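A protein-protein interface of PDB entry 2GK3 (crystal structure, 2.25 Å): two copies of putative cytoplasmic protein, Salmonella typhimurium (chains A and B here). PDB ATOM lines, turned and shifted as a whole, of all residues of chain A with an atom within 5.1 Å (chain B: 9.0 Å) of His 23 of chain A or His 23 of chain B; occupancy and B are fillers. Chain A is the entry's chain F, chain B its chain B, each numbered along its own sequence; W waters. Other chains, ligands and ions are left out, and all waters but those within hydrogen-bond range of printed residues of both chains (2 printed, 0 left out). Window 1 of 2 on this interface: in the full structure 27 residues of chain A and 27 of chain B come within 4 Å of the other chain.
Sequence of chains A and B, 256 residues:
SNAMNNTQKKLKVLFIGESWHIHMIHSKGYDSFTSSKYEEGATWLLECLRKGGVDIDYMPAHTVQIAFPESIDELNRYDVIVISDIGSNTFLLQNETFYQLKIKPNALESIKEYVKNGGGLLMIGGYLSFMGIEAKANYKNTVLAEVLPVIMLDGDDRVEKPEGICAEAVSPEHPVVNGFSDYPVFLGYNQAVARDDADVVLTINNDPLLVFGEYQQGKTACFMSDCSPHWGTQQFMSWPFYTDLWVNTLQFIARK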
ATOM      1  N   HIS A  21      16.445  15.819  12.694  1.00  0.00           N
ATOM      2  CA  HIS A  21      16.225  15.045  13.906  1.00  0.00           C
ATOM      3  C   HIS A  21      16.611  15.947  15.093  1.00  0.00           C
ATOM      4  O   HIS A  21      17.786  16.312  15.243  1.00  0.00           O
ATOM      5  CB  HIS A  21      17.087  13.757  13.890  1.00  0.00           C
ATOM      6  CG  HIS A  21      16.722  12.761  12.815  1.00  0.00           C
ATOM      7  ND1 HIS A  21      16.257  11.490  13.099  1.00  0.00           N
ATOM      8  CD2 HIS A  21      16.789  12.834  11.465  1.00  0.00           C
ATOM      9  CE1 HIS A  21      16.031  10.838  11.974  1.00  0.00           C
ATOM     10  NE2 HIS A  21      16.346  11.631  10.967  1.00  0.00           N
ATOM     11  N   ILE A  22      15.631  16.337  15.913  1.00  0.00           N
ATOM     12  CA  ILE A  22      15.878  17.183  17.069  1.00  0.00           C
ATOM     13  C   ILE A  22      16.102  16.308  18.301  1.00  0.00           C
ATOM     14  O   ILE A  22      15.326  15.401  18.578  1.00  0.00           O
ATOM     15  CB  ILE A  22      14.716  18.175  17.348  1.00  0.00           C
ATOM     16  CG1 ILE A  22      14.442  19.074  16.137  1.00  0.00           C
ATOM     17  CG2 ILE A  22      15.052  19.064  18.531  1.00  0.00           C
ATOM     18  CD1 ILE A  22      13.308  20.095  16.349  1.00  0.00           C
ATOM     19  N   HIS A  23      17.177  16.576  19.032  1.00  0.00           N
ATOM     20  CA  HIS A  23      17.362  15.978  20.335  1.00  0.00           C
ATOM     21  C   HIS A  23      17.243  17.098  21.353  1.00  0.00           C
ATOM     22  O   HIS A  23      18.021  18.031  21.323  1.00  0.00           O
ATOM     23  CB  HIS A  23      18.719  15.241  20.420  1.00  0.00           C
ATOM     24  CG  HIS A  23      19.058  14.750  21.801  1.00  0.00           C
ATOM     25  ND1 HIS A  23      18.401  13.696  22.405  1.00  0.00           N
ATOM     26  CD2 HIS A  23      19.980  15.175  22.699  1.00  0.00           C
ATOM     27  CE1 HIS A  23      18.912  13.484  23.605  1.00  0.00           C
ATOM     28  NE2 HIS A  23      19.866  14.371  23.810  1.00  0.00           N
ATOM     29  N   MET A  24      16.242  17.021  22.225  1.00  0.00           N
ATOM     30  CA  MET A  24      16.010  18.041  23.248  1.00  0.00           C
ATOM     31  C   MET A  24      16.418  17.526  24.598  1.00  0.00           C
ATOM     32  O   MET A  24      16.016  16.433  25.000  1.00  0.00           O
ATOM     33  CB  MET A  24      14.537  18.414  23.369  1.00  0.00           C
ATOM     34  CG  MET A  24      13.933  18.973  22.153  1.00  0.00           C
ATOM     35  SD  MET A  24      12.191  19.683  22.535  1.00  0.00           S
ATOM     36  CE  MET A  24      11.650  19.728  20.669  1.00  0.00           C
ATOM     37  N   ILE A  25      17.180  18.351  25.308  1.00  0.00           N
ATOM     38  CA  ILE A  25      17.644  18.060  26.650  1.00  0.00           C
ATOM     39  C   ILE A  25      16.963  19.087  27.552  1.00  0.00           C
ATOM     40  O   ILE A  25      17.288  20.252  27.487  1.00  0.00           O
ATOM     41  CB  ILE A  25      19.201  18.186  26.750  1.00  0.00           C
ATOM     42  CG1 ILE A  25      19.884  17.277  25.725  1.00  0.00           C
ATOM     43  CG2 ILE A  25      19.664  17.917  28.186  1.00  0.00           C
ATOM     44  CD1 ILE A  25      21.399  17.457  25.611  1.00  0.00           C
ATOM     45  N   THR A  34      15.385  13.775  28.392  1.00  0.00           N
ATOM     46  CA  THR A  34      15.409  14.041  26.985  1.00  0.00           C
ATOM     47  C   THR A  34      14.152  13.590  26.228  1.00  0.00           C
ATOM     48  O   THR A  34      13.406  12.694  26.663  1.00  0.00           O
ATOM     49  CB  THR A  34      16.694  13.487  26.327  1.00  0.00           C
ATOM     50  OG1 THR A  34      16.597  12.061  26.138  1.00  0.00           O
ATOM     51  CG2 THR A  34      17.944  13.847  27.171  1.00  0.00           C
ATOM     52  N   SER A  35      13.912  14.264  25.104  1.00  0.00           N
ATOM     53  CA  SER A  35      12.929  13.832  24.126  1.00  0.00           C
ATOM     54  C   SER A  35      13.504  14.097  22.749  1.00  0.00           C
ATOM     55  O   SER A  35      14.186  15.103  22.541  1.00  0.00           O
ATOM     56  CB  SER A  35      11.620  14.589  24.300  1.00  0.00           C
ATOM     57  OG  SER A  35      11.810  15.975  24.134  1.00  0.00           O
ATOM     58  N   SER A  36      13.215  13.205  21.807  1.00  0.00           N
ATOM     59  CA  SER A  36      13.730  13.352  20.463  1.00  0.00           C
ATOM     60  C   SER A  36      12.599  13.307  19.441  1.00  0.00           C
ATOM     61  O   SER A  36      11.547  12.713  19.691  1.00  0.00           O
ATOM     62  CB  SER A  36      14.805  12.307  20.199  1.00  0.00           C
ATOM     63  OG  SER A  36      15.851  12.426  21.141  1.00  0.00           O
ATOM     64  N   TRP B  20      12.435  25.319  33.219  1.00  0.00           N
ATOM     65  CA  TRP B  20      13.426  24.473  32.601  1.00  0.00           C
ATOM     66  C   TRP B  20      14.202  25.272  31.589  1.00  0.00           C
ATOM     67  O   TRP B  20      13.709  26.278  31.078  1.00  0.00           O
ATOM     68  CB  TRP B  20      12.760  23.280  31.904  1.00  0.00           C
ATOM     69  CG  TRP B  20      11.635  23.659  30.995  1.00  0.00           C
ATOM     70  CD1 TRP B  20      11.721  23.963  29.665  1.00  0.00           C
ATOM     71  CD2 TRP B  20      10.250  23.770  31.342  1.00  0.00           C
ATOM     72  NE1 TRP B  20      10.475  24.258  29.161  1.00  0.00           N
ATOM     73  CE2 TRP B  20       9.555  24.146  30.169  1.00  0.00           C
ATOM     74  CE3 TRP B  20       9.525  23.581  32.529  1.00  0.00           C
ATOM     75  CZ2 TRP B  20       8.172  24.342  30.149  1.00  0.00           C
ATOM     76  CZ3 TRP B  20       8.156  23.785  32.507  1.00  0.00           C
ATOM     77  CH2 TRP B  20       7.496  24.165  31.329  1.00  0.00           C
ATOM     78  N   HIS B  21      15.413  24.813  31.304  1.00  0.00           N
ATOM     79  CA  HIS B  21      16.164  25.316  30.187  1.00  0.00           C
ATOM     80  C   HIS B  21      16.395  24.170  29.208  1.00  0.00           C
ATOM     81  O   HIS B  21      16.959  23.131  29.575  1.00  0.00           O
ATOM     82  CB  HIS B  21      17.498  25.916  30.636  1.00  0.00           C
ATOM     83  CG  HIS B  21      18.364  26.317  29.493  1.00  0.00           C
ATOM     84  ND1 HIS B  21      19.170  25.422  28.829  1.00  0.00           N
ATOM     85  CD2 HIS B  21      18.503  27.500  28.852  1.00  0.00           C
ATOM     86  CE1 HIS B  21      19.785  26.038  27.837  1.00  0.00           C
ATOM     87  NE2 HIS B  21      19.404  27.302  27.834  1.00  0.00           N
ATOM     88  N   ILE B  22      15.972  24.372  27.966  1.00  0.00           N
ATOM     89  CA  ILE B  22      16.051  23.333  26.943  1.00  0.00           C
ATOM     90  C   ILE B  22      17.221  23.616  26.028  1.00  0.00           C
ATOM     91  O   ILE B  22      17.364  24.728  25.526  1.00  0.00           O
ATOM     92  CB  ILE B  22      14.759  23.248  26.082  1.00  0.00           C
ATOM     93  CG1 ILE B  22      13.587  22.730  26.920  1.00  0.00           C
ATOM     94  CG2 ILE B  22      14.967  22.348  24.867  1.00  0.00           C
ATOM     95  CD1 ILE B  22      12.241  22.780  26.188  1.00  0.00           C
ATOM     96  N   HIS B  23      18.052  22.605  25.820  1.00  0.00           N
ATOM     97  CA  HIS B  23      19.081  22.665  24.811  1.00  0.00           C
ATOM     98  C   HIS B  23      18.631  21.773  23.678  1.00  0.00           C
ATOM     99  O   HIS B  23      18.473  20.568  23.878  1.00  0.00           O
ATOM    100  CB  HIS B  23      20.429  22.187  25.380  1.00  0.00           C
ATOM    101  CG  HIS B  23      21.559  22.293  24.409  1.00  0.00           C
ATOM    102  ND1 HIS B  23      22.057  23.504  23.980  1.00  0.00           N
ATOM    103  CD2 HIS B  23      22.283  21.339  23.769  1.00  0.00           C
ATOM    104  CE1 HIS B  23      23.037  23.292  23.120  1.00  0.00           C
ATOM    105  NE2 HIS B  23      23.204  21.988  22.984  1.00  0.00           N
ATOM    106  N   MET B  24      18.437  22.362  22.493  1.00  0.00           N
ATOM    107  CA  MET B  24      17.954  21.647  21.302  1.00  0.00           C
ATOM    108  C   MET B  24      19.050  21.436  20.288  1.00  0.00           C
ATOM    109  O   MET B  24      19.700  22.388  19.869  1.00  0.00           O
ATOM    110  CB  MET B  24      16.851  22.437  20.608  1.00  0.00           C
ATOM    111  CG  MET B  24      15.470  22.207  21.144  1.00  0.00           C
ATOM    112  SD  MET B  24      14.125  23.172  20.142  1.00  0.00           S
ATOM    113  CE  MET B  24      13.366  23.976  21.704  1.00  0.00           C
ATOM    114  N   ILE B  25      19.218  20.201  19.848  1.00  0.00           N
ATOM    115  CA  ILE B  25      20.199  19.881  18.825  1.00  0.00           C
ATOM    116  C   ILE B  25      19.423  19.529  17.558  1.00  0.00           C
ATOM    117  O   ILE B  25      18.748  18.492  17.482  1.00  0.00           O
ATOM    118  CB  ILE B  25      21.169  18.734  19.287  1.00  0.00           C
ATOM    119  CG1 ILE B  25      21.639  18.989  20.727  1.00  0.00           C
ATOM    120  CG2 ILE B  25      22.340  18.551  18.296  1.00  0.00           C
ATOM    121  CD1 ILE B  25      22.732  18.042  21.240  1.00  0.00           C
ATOM    122  N   HIS B  26      19.496  20.418  16.567  1.00  0.00           N
ATOM    123  CA  HIS B  26      18.782  20.223  15.322  1.00  0.00           C
ATOM    124  C   HIS B  26      19.765  19.643  14.324  1.00  0.00           C
ATOM    125  O   HIS B  26      20.551  20.388  13.747  1.00  0.00           O
ATOM    126  CB  HIS B  26      18.262  21.549  14.752  1.00  0.00           C
ATOM    127  CG  HIS B  26      17.544  22.438  15.727  1.00  0.00           C
ATOM    128  ND1 HIS B  26      16.187  22.693  15.642  1.00  0.00           N
ATOM    129  CD2 HIS B  26      18.006  23.222  16.731  1.00  0.00           C
ATOM    130  CE1 HIS B  26      15.839  23.560  16.574  1.00  0.00           C
ATOM    131  NE2 HIS B  26      16.924  23.894  17.253  1.00  0.00           N
ATOM    132  N   SER B  27      19.714  18.335  14.092  1.00  0.00           N
ATOM    133  CA  SER B  27      20.586  17.704  13.092  1.00  0.00           C
ATOM    134  C   SER B  27      19.918  17.613  11.723  1.00  0.00           C
ATOM    135  O   SER B  27      18.914  16.891  11.547  1.00  0.00           O
ATOM    136  CB  SER B  27      21.053  16.305  13.531  1.00  0.00           C
ATOM    137  OG  SER B  27      21.565  16.331  14.844  1.00  0.00           O
ATOM    138  N   SER B  32      24.672  19.832  12.528  1.00  0.00           N
ATOM    139  CA  SER B  32      23.673  20.206  13.486  1.00  0.00           C
ATOM    140  C   SER B  32      23.882  21.652  13.940  1.00  0.00           C
ATOM    141  O   SER B  32      25.014  22.138  14.036  1.00  0.00           O
ATOM    142  CB  SER B  32      23.661  19.219  14.676  1.00  0.00           C
ATOM    143  OG  SER B  32      24.417  19.727  15.776  1.00  0.00           O
ATOM    144  N   PHE B  33      22.779  22.345  14.191  1.00  0.00           N
ATOM    145  CA  PHE B  33      22.831  23.631  14.863  1.00  0.00           C
ATOM    146  C   PHE B  33      21.980  23.568  16.129  1.00  0.00           C
ATOM    147  O   PHE B  33      21.077  22.729  16.257  1.00  0.00           O
ATOM    148  CB  PHE B  33      22.409  24.779  13.932  1.00  0.00           C
ATOM    149  CG  PHE B  33      20.918  24.999  13.859  1.00  0.00           C
ATOM    150  CD1 PHE B  33      20.290  25.870  14.737  1.00  0.00           C
ATOM    151  CD2 PHE B  33      20.148  24.331  12.903  1.00  0.00           C
ATOM    152  CE1 PHE B  33      18.903  26.076  14.671  1.00  0.00           C
ATOM    153  CE2 PHE B  33      18.772  24.541  12.818  1.00  0.00           C
ATOM    154  CZ  PHE B  33      18.146  25.401  13.714  1.00  0.00           C
ATOM    155  N   THR B  34      22.275  24.452  17.065  1.00  0.00           N
ATOM    156  CA  THR B  34      21.649  24.403  18.361  1.00  0.00           C
ATOM    157  C   THR B  34      20.912  25.705  18.647  1.00  0.00           C
ATOM    158  O   THR B  34      21.265  26.769  18.142  1.00  0.00           O
ATOM    159  CB  THR B  34      22.681  24.064  19.488  1.00  0.00           C
ATOM    160  OG1 THR B  34      23.742  25.039  19.514  1.00  0.00           O
ATOM    161  CG2 THR B  34      23.302  22.709  19.246  1.00  0.00           C
ATOM    162  N   SER B  35      19.837  25.597  19.415  1.00  0.00           N
ATOM    163  CA  SER B  35      19.114  26.740  19.900  1.00  0.00           C
ATOM    164  C   SER B  35      18.790  26.354  21.332  1.00  0.00           C
ATOM    165  O   SER B  35      18.481  25.193  21.606  1.00  0.00           O
ATOM    166  CB  SER B  35      17.851  26.968  19.057  1.00  0.00           C
ATOM    167  OG  SER B  35      16.906  25.891  19.165  1.00  0.00           O
ATOM    168  N   SER B  36      18.921  27.286  22.260  1.00  0.00           N
ATOM    169  CA  SER B  36      18.577  27.015  23.656  1.00  0.00           C
ATOM    170  C   SER B  36      17.421  27.889  24.074  1.00  0.00           C
ATOM    171  O   SER B  36      17.261  28.993  23.580  1.00  0.00           O
ATOM    172  CB  SER B  36      19.768  27.215  24.579  1.00  0.00           C
ATOM    173  OG  SER B  36      20.781  26.278  24.268  1.00  0.00           O
ATOM    174  N   LYS B  37      16.623  27.390  25.010  1.00  0.00           N
ATOM    175  CA  LYS B  37      15.305  27.965  25.283  1.00  0.00           C
ATOM    176  C   LYS B  37      14.941  27.807  26.756  1.00  0.00           C
ATOM    177  O   LYS B  37      14.806  26.687  27.256  1.00  0.00           O
ATOM    178  CB  LYS B  37      14.265  27.249  24.404  1.00  0.00           C
ATOM    179  CG  LYS B  37      12.824  27.738  24.559  1.00  0.00           C
ATOM    180  CD  LYS B  37      11.887  26.807  23.818  1.00  0.00           C
ATOM    181  CE  LYS B  37      10.492  27.393  23.660  1.00  0.00           C
ATOM    182  NZ  LYS B  37       9.589  26.400  22.943  1.00  0.00           N
ATOM    183  N   TYR B  38      14.773  28.925  27.446  1.00  0.00           N
ATOM    184  CA  TYR B  38      14.259  28.887  28.805  1.00  0.00           C
ATOM    185  C   TYR B  38      12.718  29.092  28.816  1.00  0.00           C
ATOM    186  O   TYR B  38      12.190  29.964  28.120  1.00  0.00           O
ATOM    187  CB  TYR B  38      14.981  29.918  29.661  1.00  0.00           C
ATOM    188  CG  TYR B  38      14.414  30.085  31.055  1.00  0.00           C
ATOM    189  CD1 TYR B  38      14.780  29.220  32.084  1.00  0.00           C
ATOM    190  CD2 TYR B  38      13.509  31.109  31.349  1.00  0.00           C
ATOM    191  CE1 TYR B  38      14.272  29.369  33.353  1.00  0.00           C
ATOM    192  CE2 TYR B  38      12.991  31.265  32.643  1.00  0.00           C
ATOM    193  CZ  TYR B  38      13.385  30.391  33.627  1.00  0.00           C
ATOM    194  OH  TYR B  38      12.891  30.513  34.900  1.00  0.00           O
HETATM  195  O   HOH W   1      20.218  15.937  16.937  1.00  0.00           O
HETATM  196  O   HOH W   2      19.566  21.657  29.076  1.00  0.00           O
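The backbone carbonyl oxygen (O) of His 23 of chain B sits at hydrogen-bond distance from the backbone NH (N) of Ile 25 of chain A, 2.9 Å away. The backbone NH of Ile 25 of chain B sits at hydrogen-bond distance from the backbone carbonyl oxygen of His 23 of chain A, 2.9 Å away. The backbone NH of His 21 of chain A lies within hydrogen-bond range of the backbone carbonyl oxygen of Ser 27 of chain B. O of Ile 25 of chain B lies close to O of His 21 of chain A (3.3 Å).
N of Ile 22 of chain B is in hydrogen-bond range of O of Lys 37 of chain B. ND1 of His 23 of chain B is in hydrogen-bond range of OG of Ser 36 of chain B (3.1 Å). The backbone NH (N) of Met 24 of chain B lies within hydrogen-bond range of the backbone carbonyl oxygen (O) of Ser 35 of chain B (3.0 Å). The backbone carbonyl oxygen of Phe 33 of chain B is in hydrogen-bond range of the backbone NH of His 26 of chain B, 2.8 Å away. A ring nitrogen (NE2) of His 26 of chain B sits at hydrogen-bond distance from the side-chain hydroxyl (OG) of Ser 35 of chain B, at 2.8 Å. N of Met 24 of chain A lies within hydrogen-bond range of O of Ser 35 of chain A, 2.8 Å away.
Among the printed residues, pairs that only touch across the chains: His 21 of chain A with His 26 of chain B (3.98 Å), Ile 22 of chain A with Ile 25 of chain B (3.2 Å), Ile 22 of chain A with His 26 of chain B (3.9 Å), His 23 of chain A with His 23 of chain B (3.6 Å), His 23 of chain A with Met 24 of chain B (3.6 Å), Met 24 of chain A with His 23 of chain B (3.6 Å), Met 24 of chain A with Met 24 of chain B (3.7 Å), Ile 25 of chain A with His 21 of chain B (3.6 Å) and Ile 25 of chain A with Ile 22 of chain B (3.4 Å).
His 23 of chain B touches three residues of chain A. Of the printed residues of chain B, Ile 25 of chain A touches His 21, Ile 22 and His 23. Printed residues of chain A within 4 Å of Ile 22 of chain B: Ile 25 (3.4 Å). Of the printed residues of chain B, Met 24 of chain A touches His 23 and Met 24. Phe 33 of chain B touches none of the printed residues of chain A. The nearest printed residue of chain A that does not touch His 23 of chain B is Ile 22 of chain A (6.5 Å). The nearest printed residue of chain A that does not touch His 21 of chain B is Met 24 of chain A (7.5 Å).
Of the 8 printed residues of chain A, 5 touch a printed residue of chain B. Hydrophobic or aromatic side chains of chain A that line the printed part of chain B: Ile 22, Met 24 and Ile 25. Of the 15 printed residues of chain B, 7 touch a printed residue of chain A. Hydrophobic or aromatic side chains of chain B that line the printed part of chain A: Met 24, Ile 25 and His 26. Along chain B the printed residues that touch a printed residue of chain A span positions 21 to 27. Among the printed residues, no Asp or Glu carboxylate lies within 4 Å of a Lys or Arg side-chain nitrogen of the other chain.
His 21 of chain A touches Ile 25 of chain B, and with the chains exchanged Ile 25 of chain A touches His 21 of chain B. Ile 22 of chain A touches Ile 25 of chain B, and with the chains exchanged Ile 25 of chain A touches Ile 22 of chain B. His 23 of chain B touches its own counterpart, His 23 of chain A. His 23 of chain A touches Ile 25 of chain B, and with the chains exchanged Ile 25 of chain A touches His 23 of chain B. Positions printed for both chains: 21, 22, 23, 24, 25, 34, 35 and 36. Of the 13 pairs that touch across the chains among the printed residues, 10 have their exchanged pair printed and touching as well.
Water W1 lies within hydrogen-bond range of the side-chain hydroxyl of Ser 27 of chain B, the backbone carbonyl oxygen of His 21 of chain A and the backbone carbonyl oxygen of Ile 25 of chain B. Water W2 lies within hydrogen-bond range of O of His 21 of chain B (3.0 Å) and O of Ile 25 of chain A (3.1 Å).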
